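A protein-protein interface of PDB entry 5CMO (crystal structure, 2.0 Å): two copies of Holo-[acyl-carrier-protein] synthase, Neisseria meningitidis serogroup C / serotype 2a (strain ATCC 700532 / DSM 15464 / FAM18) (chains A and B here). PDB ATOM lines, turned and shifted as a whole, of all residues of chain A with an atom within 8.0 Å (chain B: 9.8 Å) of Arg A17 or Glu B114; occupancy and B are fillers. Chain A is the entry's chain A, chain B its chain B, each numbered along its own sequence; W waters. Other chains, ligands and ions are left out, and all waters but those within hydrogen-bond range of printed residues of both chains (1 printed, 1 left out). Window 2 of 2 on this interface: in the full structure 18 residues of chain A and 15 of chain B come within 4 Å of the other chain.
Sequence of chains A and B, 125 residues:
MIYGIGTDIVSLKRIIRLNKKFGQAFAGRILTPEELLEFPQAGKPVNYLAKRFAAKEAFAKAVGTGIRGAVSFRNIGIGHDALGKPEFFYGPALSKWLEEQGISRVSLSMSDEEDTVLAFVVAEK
Ile A16 touches none of the printed residues of chain B. Leu A18 touches none of the printed residues of chain B. Of the printed residues of chain A, Ser B111 touches Ile A9 (3.6 Å). Of chain A, only Arg A17 (3.0 Å) comes within 4 Å of Glu B114. Of the printed residues of chain A, Leu B118 touches Ile A9 (3.6 Å). The nearest residue of chain B that does not touch Arg A17 is Glu B113 (6.6 Å). The nearest printed residue of chain B that does not touch Ile A9 is Asp B112 (4.01 Å).
Ser B111 touches Ile A9 (OG to N, 3.6 Å). Ile A9 touches Glu B113. CG2 of Thr B116 touches CD1 of Ile A9 (3.7 Å). CD2 of Leu B118 touches CG2 of Ile A9, at 3.6 Å. Glu B113 touches Val A10. Glu B113 touches Arg A14.
The side-chain hydroxyl (OG) of Ser A11 is in hydrogen-bond range of the side-chain carboxylate (OD2) of Asp A115. The backbone NH of Arg A14 sits at hydrogen-bond distance from the side-chain hydroxyl of Ser A11 (3.4 Å). N of Lys A13 lies close to OG of Ser A11. O of Ser B111 sits at hydrogen-bond distance from N of Leu B118, 2.9 Å away.
Printed residues of chain A that touch a printed residue of chain B: Ile A9, Val A10, Ser A11, Arg A14 and Arg A17. Hydrophobic or aromatic side chains of chain A that line the printed part of chain B: Ile A9. Of the 19 printed residues of chain B, 5 touch a printed residue of chain A. Printed residues of chain B that touch a printed residue of chain A: Ser B111, Glu B113, Glu B114, Thr B116 and Leu B118. Hydrophobic or aromatic side chains of chain B within 4 Å of the printed part of chain A: Leu B118. Among the printed residues, 8 pairs touch across the chains.
N of Ser A11 lies within hydrogen-bond range of OE2 of Glu B113. The side-chain carboxylate (OE2) of Glu B114 is in salt-bridge range of the guanidinium group (NH2) of Arg A17, at 3.0 Å.
Water W1 lies within hydrogen-bond range of OE2 of Glu B114, NH2 of Arg A17 and OG of Ser A11.
8 positions are printed for both chains. Of the 8 pairs that touch across the chains among the printed residues, none has its exchanged pair printed and touching as well.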
ATOM      1  N   ILE A   9      -7.501   8.038  10.823  1.00  0.00           N
ATOM      2  CA  ILE A   9      -8.402   8.182  11.958  1.00  0.00           C
ATOM      3  C   ILE A   9      -8.187   7.011  12.907  1.00  0.00           C
ATOM      4  O   ILE A   9      -7.984   5.875  12.471  1.00  0.00           O
ATOM      5  CB  ILE A   9      -9.878   8.260  11.513  1.00  0.00           C
ATOM      6  CG1 ILE A   9     -10.177   7.189  10.460  1.00  0.00           C
ATOM      7  CG2 ILE A   9     -10.181   9.645  10.953  1.00  0.00           C
ATOM      8  CD1 ILE A   9     -11.624   7.139  10.026  1.00  0.00           C
ATOM      9  N   VAL A  10      -8.209   7.303  14.204  1.00  0.00           N
ATOM     10  CA  VAL A  10      -7.950   6.299  15.227  1.00  0.00           C
ATOM     11  C   VAL A  10      -9.006   6.366  16.323  1.00  0.00           C
ATOM     12  O   VAL A  10      -9.354   7.447  16.805  1.00  0.00           O
ATOM     13  CB  VAL A  10      -6.546   6.477  15.849  1.00  0.00           C
ATOM     14  CG1 VAL A  10      -6.347   5.531  17.029  1.00  0.00           C
ATOM     15  CG2 VAL A  10      -5.467   6.245  14.799  1.00  0.00           C
ATOM     16  N   SER A  11      -9.503   5.198  16.711  1.00  0.00           N
ATOM     17  CA  SER A  11     -10.465   5.085  17.795  1.00  0.00           C
ATOM     18  C   SER A  11      -9.737   4.933  19.123  1.00  0.00           C
ATOM     19  O   SER A  11      -8.833   4.108  19.247  1.00  0.00           O
ATOM     20  CB  SER A  11     -11.397   3.897  17.558  1.00  0.00           C
ATOM     21  OG  SER A  11     -12.092   3.552  18.741  1.00  0.00           O
ATOM     22  N   LEU A  12     -10.125   5.735  20.110  1.00  0.00           N
ATOM     23  CA  LEU A  12      -9.524   5.653  21.436  1.00  0.00           C
ATOM     24  C   LEU A  12      -9.704   4.257  22.021  1.00  0.00           C
ATOM     25  O   LEU A  12      -8.820   3.743  22.702  1.00  0.00           O
ATOM     26  CB  LEU A  12     -10.132   6.692  22.381  1.00  0.00           C
ATOM     27  CG  LEU A  12      -9.835   8.169  22.110  1.00  0.00           C
ATOM     28  CD1 LEU A  12     -10.450   9.025  23.206  1.00  0.00           C
ATOM     29  CD2 LEU A  12      -8.338   8.434  22.004  1.00  0.00           C
ATOM     30  N   LYS A  13     -10.851   3.645  21.742  1.00  0.00           N
ATOM     31  CA  LYS A  13     -11.165   2.332  22.288  1.00  0.00           C
ATOM     32  C   LYS A  13     -10.298   1.242  21.666  1.00  0.00           C
ATOM     33  O   LYS A  13      -9.946   0.271  22.333  1.00  0.00           O
ATOM     34  CB  LYS A  13     -12.648   2.014  22.088  1.00  0.00           C
ATOM     35  CG  LYS A  13     -13.562   2.843  22.978  1.00  0.00           C
ATOM     36  CD  LYS A  13     -15.033   2.543  22.745  1.00  0.00           C
ATOM     37  CE  LYS A  13     -15.915   3.474  23.567  1.00  0.00           C
ATOM     38  NZ  LYS A  13     -15.622   3.385  25.026  1.00  0.00           N
ATOM     39  N   ARG A  14      -9.947   1.422  20.401  1.00  0.00           N
ATOM     40  CA  ARG A  14      -9.068   0.492  19.715  1.00  0.00           C
ATOM     41  C   ARG A  14      -7.677   0.522  20.363  1.00  0.00           C
ATOM     42  O   ARG A  14      -7.043  -0.510  20.556  1.00  0.00           O
ATOM     43  CB  ARG A  14      -8.986   0.816  18.232  1.00  0.00           C
ATOM     44  CG  ARG A  14      -7.934   0.004  17.522  1.00  0.00           C
ATOM     45  CD  ARG A  14      -8.291  -0.270  16.079  1.00  0.00           C
ATOM     46  NE  ARG A  14      -7.609  -1.469  15.630  1.00  0.00           N
ATOM     47  CZ  ARG A  14      -6.470  -1.458  14.962  1.00  0.00           C
ATOM     48  NH1 ARG A  14      -5.917  -0.300  14.641  1.00  0.00           N
ATOM     49  NH2 ARG A  14      -5.902  -2.599  14.605  1.00  0.00           N
ATOM     50  N   ILE A  15      -7.217   1.717  20.704  1.00  0.00           N
ATOM     51  CA  ILE A  15      -5.931   1.886  21.375  1.00  0.00           C
ATOM     52  C   ILE A  15      -5.936   1.140  22.708  1.00  0.00           C
ATOM     53  O   ILE A  15      -4.961   0.475  23.058  1.00  0.00           O
ATOM     54  CB  ILE A  15      -5.607   3.380  21.616  1.00  0.00           C
ATOM     55  CG1 ILE A  15      -5.449   4.120  20.283  1.00  0.00           C
ATOM     56  CG2 ILE A  15      -4.344   3.540  22.463  1.00  0.00           C
ATOM     57  CD1 ILE A  15      -4.251   3.681  19.453  1.00  0.00           C
ATOM     58  N   ILE A  16      -7.040   1.254  23.440  1.00  0.00           N
ATOM     59  CA  ILE A  16      -7.186   0.584  24.727  1.00  0.00           C
ATOM     60  C   ILE A  16      -7.052  -0.927  24.569  1.00  0.00           C
ATOM     61  O   ILE A  16      -6.437  -1.591  25.401  1.00  0.00           O
ATOM     62  CB  ILE A  16      -8.547   0.918  25.382  1.00  0.00           C
ATOM     63  CG1 ILE A  16      -8.598   2.399  25.768  1.00  0.00           C
ATOM     64  CG2 ILE A  16      -8.786   0.052  26.621  1.00  0.00           C
ATOM     65  CD1 ILE A  16      -9.962   2.880  26.237  1.00  0.00           C
ATOM     66  N   ARG A  17      -7.664  -1.457  23.515  1.00  0.00           N
ATOM     67  CA  ARG A  17      -7.598  -2.881  23.212  1.00  0.00           C
ATOM     68  C   ARG A  17      -6.183  -3.308  22.823  1.00  0.00           C
ATOM     69  O   ARG A  17      -5.719  -4.377  23.213  1.00  0.00           O
ATOM     70  CB  ARG A  17      -8.609  -3.254  22.127  1.00  0.00           C
ATOM     71  CG  ARG A  17      -9.983  -3.573  22.693  1.00  0.00           C
ATOM     72  CD  ARG A  17     -10.981  -3.976  21.622  1.00  0.00           C
ATOM     73  NE  ARG A  17     -11.640  -2.822  21.022  1.00  0.00           N
ATOM     74  CZ  ARG A  17     -11.525  -2.477  19.746  1.00  0.00           C
ATOM     75  NH1 ARG A  17     -10.784  -3.205  18.925  1.00  0.00           N
ATOM     76  NH2 ARG A  17     -12.161  -1.408  19.289  1.00  0.00           N
ATOM     77  N   LEU A  18      -5.505  -2.462  22.051  1.00  0.00           N
ATOM     78  CA  LEU A  18      -4.140  -2.738  21.619  1.00  0.00           C
ATOM     79  C   LEU A  18      -3.192  -2.766  22.816  1.00  0.00           C
ATOM     80  O   LEU A  18      -2.293  -3.603  22.884  1.00  0.00           O
ATOM     81  CB  LEU A  18      -3.682  -1.696  20.596  1.00  0.00           C
ATOM     82  CG  LEU A  18      -4.271  -1.859  19.191  1.00  0.00           C
ATOM     83  CD1 LEU A  18      -4.035  -0.610  18.360  1.00  0.00           C
ATOM     84  CD2 LEU A  18      -3.674  -3.074  18.499  1.00  0.00           C
ATOM     85  N   ASN A  19      -3.397  -1.847  23.756  1.00  0.00           N
ATOM     86  CA  ASN A  19      -2.648  -1.855  25.008  1.00  0.00           C
ATOM     87  C   ASN A  19      -2.953  -3.122  25.796  1.00  0.00           C
ATOM     88  O   ASN A  19      -2.064  -3.725  26.398  1.00  0.00           O
ATOM     89  CB  ASN A  19      -2.979  -0.621  25.854  1.00  0.00           C
ATOM     90  CG  ASN A  19      -2.296   0.639  25.354  1.00  0.00           C
ATOM     91  OD1 ASN A  19      -1.257   0.581  24.697  1.00  0.00           O
ATOM     92  ND2 ASN A  19      -2.875   1.791  25.677  1.00  0.00           N
ATOM     93  N   LYS A  20      -4.222  -3.513  25.786  1.00  0.00           N
ATOM     94  CA  LYS A  20      -4.666  -4.719  26.475  1.00  0.00           C
ATOM     95  C   LYS A  20      -3.983  -5.952  25.900  1.00  0.00           C
ATOM     96  O   LYS A  20      -3.535  -6.830  26.638  1.00  0.00           O
ATOM     97  CB  LYS A  20      -6.184  -4.872  26.363  1.00  0.00           C
ATOM     98  CG  LYS A  20      -6.894  -5.047  27.697  1.00  0.00           C
ATOM     99  CD  LYS A  20      -8.277  -5.664  27.532  1.00  0.00           C
ATOM    100  CE  LYS A  20      -8.193  -7.112  27.069  1.00  0.00           C
ATOM    101  NZ  LYS A  20      -9.481  -7.838  27.231  1.00  0.00           N
ATOM    102  N   LYS A  21      -3.902  -6.005  24.575  1.00  0.00           N
ATOM    103  CA  LYS A  21      -3.372  -7.174  23.885  1.00  0.00           C
ATOM    104  C   LYS A  21      -1.857  -7.305  24.033  1.00  0.00           C
ATOM    105  O   LYS A  21      -1.351  -8.393  24.310  1.00  0.00           O
ATOM    106  CB  LYS A  21      -3.741  -7.121  22.399  1.00  0.00           C
ATOM    107  CG  LYS A  21      -3.378  -8.384  21.627  1.00  0.00           C
ATOM    108  CD  LYS A  21      -3.666  -8.245  20.138  1.00  0.00           C
ATOM    109  CE  LYS A  21      -4.818  -9.135  19.696  1.00  0.00           C
ATOM    110  NZ  LYS A  21      -4.817  -9.352  18.223  1.00  0.00           N
ATOM    111  N   PHE A  22      -1.141  -6.197  23.857  1.00  0.00           N
ATOM    112  CA  PHE A  22       0.315  -6.232  23.741  1.00  0.00           C
ATOM    113  C   PHE A  22       1.061  -5.621  24.927  1.00  0.00           C
ATOM    114  O   PHE A  22       2.279  -5.765  25.034  1.00  0.00           O
ATOM    115  CB  PHE A  22       0.749  -5.509  22.465  1.00  0.00           C
ATOM    116  CG  PHE A  22       0.378  -6.232  21.204  1.00  0.00           C
ATOM    117  CD1 PHE A  22       0.916  -7.476  20.921  1.00  0.00           C
ATOM    118  CD2 PHE A  22      -0.498  -5.663  20.296  1.00  0.00           C
ATOM    119  CE1 PHE A  22       0.579  -8.145  19.760  1.00  0.00           C
ATOM    120  CE2 PHE A  22      -0.836  -6.325  19.132  1.00  0.00           C
ATOM    121  CZ  PHE A  22      -0.297  -7.567  18.863  1.00  0.00           C
ATOM    122  N   GLY A  23       0.344  -4.942  25.813  1.00  0.00           N
ATOM    123  CA  GLY A  23       0.991  -4.223  26.897  1.00  0.00           C
ATOM    124  C   GLY A  23       1.761  -3.036  26.353  1.00  0.00           C
ATOM    125  O   GLY A  23       1.276  -2.334  25.465  1.00  0.00           O
ATOM    126  N   PHE A  26       3.211  -2.436  22.395  1.00  0.00           N
ATOM    127  CA  PHE A  26       2.566  -1.586  21.402  1.00  0.00           C
ATOM    128  C   PHE A  26       3.158  -0.183  21.426  1.00  0.00           C
ATOM    129  O   PHE A  26       3.556   0.350  20.392  1.00  0.00           O
ATOM    130  CB  PHE A  26       1.058  -1.519  21.645  1.00  0.00           C
ATOM    131  CG  PHE A  26       0.343  -0.546  20.749  1.00  0.00           C
ATOM    132  CD1 PHE A  26       0.332  -0.731  19.377  1.00  0.00           C
ATOM    133  CD2 PHE A  26      -0.316   0.552  21.277  1.00  0.00           C
ATOM    134  CE1 PHE A  26      -0.322   0.160  18.547  1.00  0.00           C
ATOM    135  CE2 PHE A  26      -0.974   1.446  20.453  1.00  0.00           C
ATOM    136  CZ  PHE A  26      -0.976   1.250  19.086  1.00  0.00           C
ATOM    137  N   VAL A  46      -3.721   7.089  26.710  1.00  0.00           N
ATOM    138  CA  VAL A  46      -4.491   6.567  25.585  1.00  0.00           C
ATOM    139  C   VAL A  46      -4.589   7.609  24.476  1.00  0.00           C
ATOM    140  O   VAL A  46      -4.389   7.299  23.301  1.00  0.00           O
ATOM    141  CB  VAL A  46      -5.905   6.139  26.019  1.00  0.00           C
ATOM    142  CG1 VAL A  46      -6.702   5.620  24.828  1.00  0.00           C
ATOM    143  CG2 VAL A  46      -5.824   5.074  27.100  1.00  0.00           C
ATOM    144  N   ASP A 115     -14.556   9.657  20.708  1.00  0.00           N
ATOM    145  CA  ASP A 115     -13.732   8.469  20.522  1.00  0.00           C
ATOM    146  C   ASP A 115     -12.785   8.583  19.327  1.00  0.00           C
ATOM    147  O   ASP A 115     -11.803   7.847  19.231  1.00  0.00           O
ATOM    148  CB  ASP A 115     -14.635   7.248  20.354  1.00  0.00           C
ATOM    149  CG  ASP A 115     -13.854   5.966  20.187  1.00  0.00           C
ATOM    150  OD1 ASP A 115     -13.135   5.578  21.132  1.00  0.00           O
ATOM    151  OD2 ASP A 115     -13.957   5.344  19.110  1.00  0.00           O
ATOM    152  N   ILE B   9     -16.907  11.536   4.276  1.00  0.00           N
ATOM    153  CA  ILE B   9     -16.981  10.428   5.221  1.00  0.00           C
ATOM    154  C   ILE B   9     -18.082   9.473   4.785  1.00  0.00           C
ATOM    155  O   ILE B   9     -19.190   9.903   4.453  1.00  0.00           O
ATOM    156  CB  ILE B   9     -17.270  10.908   6.660  1.00  0.00           C
ATOM    157  CG1 ILE B   9     -16.098  11.723   7.212  1.00  0.00           C
ATOM    158  CG2 ILE B   9     -17.550   9.716   7.575  1.00  0.00           C
ATOM    159  CD1 ILE B   9     -14.880  10.896   7.592  1.00  0.00           C
ATOM    160  N   VAL B  10     -17.774   8.180   4.799  1.00  0.00           N
ATOM    161  CA  VAL B  10     -18.734   7.154   4.414  1.00  0.00           C
ATOM    162  C   VAL B  10     -18.761   6.040   5.450  1.00  0.00           C
ATOM    163  O   VAL B  10     -17.721   5.516   5.851  1.00  0.00           O
ATOM    164  CB  VAL B  10     -18.404   6.561   3.026  1.00  0.00           C
ATOM    165  CG1 VAL B  10     -19.330   5.391   2.698  1.00  0.00           C
ATOM    166  CG2 VAL B  10     -18.514   7.632   1.955  1.00  0.00           C
ATOM    167  N   SER B  11     -19.969   5.689   5.874  1.00  0.00           N
ATOM    168  CA  SER B  11     -20.180   4.582   6.792  1.00  0.00           C
ATOM    169  C   SER B  11     -20.236   3.266   6.024  1.00  0.00           C
ATOM    170  O   SER B  11     -20.908   3.174   4.996  1.00  0.00           O
ATOM    171  CB  SER B  11     -21.476   4.787   7.580  1.00  0.00           C
ATOM    172  OG  SER B  11     -21.843   3.611   8.272  1.00  0.00           O
ATOM    173  N   LEU B  12     -19.528   2.254   6.518  1.00  0.00           N
ATOM    174  CA  LEU B  12     -19.608   0.919   5.933  1.00  0.00           C
ATOM    175  C   LEU B  12     -21.050   0.427   5.942  1.00  0.00           C
ATOM    176  O   LEU B  12     -21.495  -0.234   5.004  1.00  0.00           O
ATOM    177  CB  LEU B  12     -18.717  -0.067   6.692  1.00  0.00           C
ATOM    178  CG  LEU B  12     -17.208   0.180   6.690  1.00  0.00           C
ATOM    179  CD1 LEU B  12     -16.500  -0.963   7.400  1.00  0.00           C
ATOM    180  CD2 LEU B  12     -16.669   0.339   5.281  1.00  0.00           C
ATOM    181  N   LYS B  13     -21.774   0.761   7.006  1.00  0.00           N
ATOM    182  CA  LYS B  13     -23.174   0.371   7.138  1.00  0.00           C
ATOM    183  C   LYS B  13     -24.022   0.930   5.999  1.00  0.00           C
ATOM    184  O   LYS B  13     -24.920   0.254   5.501  1.00  0.00           O
ATOM    185  CB  LYS B  13     -23.730   0.834   8.490  1.00  0.00           C
ATOM    186  CG  LYS B  13     -23.176   0.060   9.677  1.00  0.00           C
ATOM    187  CD  LYS B  13     -23.787   0.505  10.999  1.00  0.00           C
ATOM    188  CE  LYS B  13     -23.391   1.928  11.355  1.00  0.00           C
ATOM    189  NZ  LYS B  13     -23.385   2.154  12.828  1.00  0.00           N
ATOM    190  N   ILE B  16     -23.308  -1.171   2.968  1.00  0.00           N
ATOM    191  CA  ILE B  16     -23.957  -2.467   3.132  1.00  0.00           C
ATOM    192  C   ILE B  16     -25.441  -2.370   2.786  1.00  0.00           C
ATOM    193  O   ILE B  16     -25.984  -3.239   2.103  1.00  0.00           O
ATOM    194  CB  ILE B  16     -23.782  -3.000   4.571  1.00  0.00           C
ATOM    195  CG1 ILE B  16     -22.317  -3.369   4.813  1.00  0.00           C
ATOM    196  CG2 ILE B  16     -24.665  -4.228   4.820  1.00  0.00           C
ATOM    197  CD1 ILE B  16     -21.975  -3.667   6.266  1.00  0.00           C
ATOM    198  N   LYS B  44     -11.391  -7.010   1.379  1.00  0.00           N
ATOM    199  CA  LYS B  44     -12.596  -6.565   2.071  1.00  0.00           C
ATOM    200  C   LYS B  44     -13.482  -5.802   1.087  1.00  0.00           C
ATOM    201  O   LYS B  44     -13.343  -4.587   0.939  1.00  0.00           O
ATOM    202  CB  LYS B  44     -12.237  -5.696   3.282  1.00  0.00           C
ATOM    203  CG  LYS B  44     -11.290  -6.385   4.261  1.00  0.00           C
ATOM    204  CD  LYS B  44     -11.415  -5.834   5.677  1.00  0.00           C
ATOM    205  CE  LYS B  44     -11.040  -4.363   5.757  1.00  0.00           C
ATOM    206  NZ  LYS B  44      -9.670  -4.093   5.239  1.00  0.00           N
ATOM    207  N   VAL B  46     -16.564  -4.723   1.019  1.00  0.00           N
ATOM    208  CA  VAL B  46     -17.330  -3.584   1.524  1.00  0.00           C
ATOM    209  C   VAL B  46     -16.440  -2.346   1.657  1.00  0.00           C
ATOM    210  O   VAL B  46     -16.810  -1.252   1.218  1.00  0.00           O
ATOM    211  CB  VAL B  46     -17.983  -3.901   2.886  1.00  0.00           C
ATOM    212  CG1 VAL B  46     -18.757  -2.696   3.408  1.00  0.00           C
ATOM    213  CG2 VAL B  46     -18.905  -5.098   2.761  1.00  0.00           C
ATOM    214  N   ASN B  47     -15.273  -2.523   2.267  1.00  0.00           N
ATOM    215  CA  ASN B  47     -14.298  -1.442   2.392  1.00  0.00           C
ATOM    216  C   ASN B  47     -13.800  -0.959   1.036  1.00  0.00           C
ATOM    217  O   ASN B  47     -13.573   0.235   0.833  1.00  0.00           O
ATOM    218  CB  ASN B  47     -13.109  -1.894   3.238  1.00  0.00           C
ATOM    219  CG  ASN B  47     -13.403  -1.852   4.722  1.00  0.00           C
ATOM    220  OD1 ASN B  47     -14.145  -2.685   5.244  1.00  0.00           O
ATOM    221  ND2 ASN B  47     -12.811  -0.886   5.413  1.00  0.00           N
ATOM    222  N   ALA B  50     -16.534   1.219  -0.215  1.00  0.00           N
ATOM    223  CA  ALA B  50     -16.679   2.394   0.645  1.00  0.00           C
ATOM    224  C   ALA B  50     -15.590   3.423   0.356  1.00  0.00           C
ATOM    225  O   ALA B  50     -15.863   4.624   0.277  1.00  0.00           O
ATOM    226  CB  ALA B  50     -16.643   1.985   2.112  1.00  0.00           C
ATOM    227  N   LYS B  51     -14.362   2.938   0.197  1.00  0.00           N
ATOM    228  CA  LYS B  51     -13.217   3.786  -0.121  1.00  0.00           C
ATOM    229  C   LYS B  51     -13.405   4.511  -1.452  1.00  0.00           C
ATOM    230  O   LYS B  51     -13.192   5.721  -1.539  1.00  0.00           O
ATOM    231  CB  LYS B  51     -11.931   2.951  -0.160  1.00  0.00           C
ATOM    232  CG  LYS B  51     -11.380   2.590   1.211  1.00  0.00           C
ATOM    233  CD  LYS B  51     -10.285   1.529   1.130  1.00  0.00           C
ATOM    234  CE  LYS B  51      -9.040   2.037   0.413  1.00  0.00           C
ATOM    235  NZ  LYS B  51      -7.882   1.115   0.594  1.00  0.00           N
ATOM    236  N   SER B 111      -8.397   6.683   4.408  1.00  0.00           N
ATOM    237  CA  SER B 111      -8.174   5.937   5.635  1.00  0.00           C
ATOM    238  C   SER B 111      -9.489   5.370   6.141  1.00  0.00           C
ATOM    239  O   SER B 111     -10.565   5.757   5.680  1.00  0.00           O
ATOM    240  CB  SER B 111      -7.538   6.815   6.708  1.00  0.00           C
ATOM    241  OG  SER B 111      -7.210   6.044   7.850  1.00  0.00           O
ATOM    242  N   ASP B 112      -9.393   4.450   7.093  1.00  0.00           N
ATOM    243  CA  ASP B 112     -10.569   3.828   7.674  1.00  0.00           C
ATOM    244  C   ASP B 112     -10.305   3.417   9.114  1.00  0.00           C
ATOM    245  O   ASP B 112      -9.179   3.078   9.483  1.00  0.00           O
ATOM    246  CB  ASP B 112     -10.992   2.612   6.852  1.00  0.00           C
ATOM    247  CG  ASP B 112      -9.981   1.488   6.918  1.00  0.00           C
ATOM    248  OD1 ASP B 112      -8.961   1.562   6.201  1.00  0.00           O
ATOM    249  OD2 ASP B 112     -10.203   0.531   7.689  1.00  0.00           O
ATOM    250  N   GLU B 113     -11.347   3.488   9.926  1.00  0.00           N
ATOM    251  CA  GLU B 113     -11.287   3.041  11.306  1.00  0.00           C
ATOM    252  C   GLU B 113     -12.635   2.398  11.580  1.00  0.00           C
ATOM    253  O   GLU B 113     -13.626   3.097  11.768  1.00  0.00           O
ATOM    254  CB  GLU B 113     -11.009   4.194  12.267  1.00  0.00           C
ATOM    255  CG  GLU B 113     -10.885   3.779  13.728  1.00  0.00           C
ATOM    256  CD  GLU B 113      -9.621   2.988  14.027  1.00  0.00           C
ATOM    257  OE1 GLU B 113      -8.990   2.472  13.087  1.00  0.00           O
ATOM    258  OE2 GLU B 113      -9.260   2.879  15.212  1.00  0.00           O
ATOM    259  N   GLU B 114     -12.672   1.075  11.590  1.00  0.00           N
ATOM    260  CA  GLU B 114     -13.917   0.367  11.832  1.00  0.00           C
ATOM    261  C   GLU B 114     -14.980   0.801  10.808  1.00  0.00           C
ATOM    262  O   GLU B 114     -14.752   0.708   9.607  1.00  0.00           O
ATOM    263  CB  GLU B 114     -14.355   0.512  13.293  1.00  0.00           C
ATOM    264  CG  GLU B 114     -13.498  -0.336  14.222  1.00  0.00           C
ATOM    265  CD  GLU B 114     -13.607   0.049  15.684  1.00  0.00           C
ATOM    266  OE1 GLU B 114     -14.342   1.003  16.009  1.00  0.00           O
ATOM    267  OE2 GLU B 114     -12.944  -0.608  16.512  1.00  0.00           O
ATOM    268  N   ASP B 115     -16.133   1.257  11.277  1.00  0.00           N
ATOM    269  CA  ASP B 115     -17.229   1.668  10.398  1.00  0.00           C
ATOM    270  C   ASP B 115     -17.007   2.938   9.580  1.00  0.00           C
ATOM    271  O   ASP B 115     -17.741   3.189   8.634  1.00  0.00           O
ATOM    272  CB  ASP B 115     -18.516   1.850  11.208  1.00  0.00           C
ATOM    273  CG  ASP B 115     -19.716   2.173  10.335  1.00  0.00           C
ATOM    274  OD1 ASP B 115     -20.039   1.368   9.443  1.00  0.00           O
ATOM    275  OD2 ASP B 115     -20.341   3.232  10.544  1.00  0.00           O
ATOM    276  N   THR B 116     -16.037   3.758   9.961  1.00  0.00           N
ATOM    277  CA  THR B 116     -15.829   5.035   9.289  1.00  0.00           C
ATOM    278  C   THR B 116     -14.755   4.946   8.213  1.00  0.00           C
ATOM    279  O   THR B 116     -13.641   4.490   8.468  1.00  0.00           O
ATOM    280  CB  THR B 116     -15.434   6.131  10.296  1.00  0.00           C
ATOM    281  OG1 THR B 116     -16.463   6.267  11.282  1.00  0.00           O
ATOM    282  CG2 THR B 116     -15.236   7.467   9.592  1.00  0.00           C
ATOM    283  N   VAL B 117     -15.110   5.389   7.011  1.00  0.00           N
ATOM    284  CA  VAL B 117     -14.166   5.510   5.908  1.00  0.00           C
ATOM    285  C   VAL B 117     -14.062   6.984   5.531  1.00  0.00           C
ATOM    286  O   VAL B 117     -15.070   7.689   5.485  1.00  0.00           O
ATOM    287  CB  VAL B 117     -14.600   4.672   4.692  1.00  0.00           C
ATOM    288  CG1 VAL B 117     -13.710   4.959   3.494  1.00  0.00           C
ATOM    289  CG2 VAL B 117     -14.564   3.191   5.036  1.00  0.00           C
ATOM    290  N   LEU B 118     -12.844   7.435   5.253  1.00  0.00           N
ATOM    291  CA  LEU B 118     -12.566   8.852   5.053  1.00  0.00           C
ATOM    292  C   LEU B 118     -11.669   9.073   3.838  1.00  0.00           C
ATOM    293  O   LEU B 118     -10.726   8.318   3.619  1.00  0.00           O
ATOM    294  CB  LEU B 118     -11.914   9.425   6.314  1.00  0.00           C
ATOM    295  CG  LEU B 118     -11.214  10.783   6.277  1.00  0.00           C
ATOM    296  CD1 LEU B 118     -12.099  11.903   5.755  1.00  0.00           C
ATOM    297  CD2 LEU B 118     -10.738  11.109   7.681  1.00  0.00           C
HETATM  298  O   HOH W   1     -13.231   0.850  18.626  1.00  0.00           O
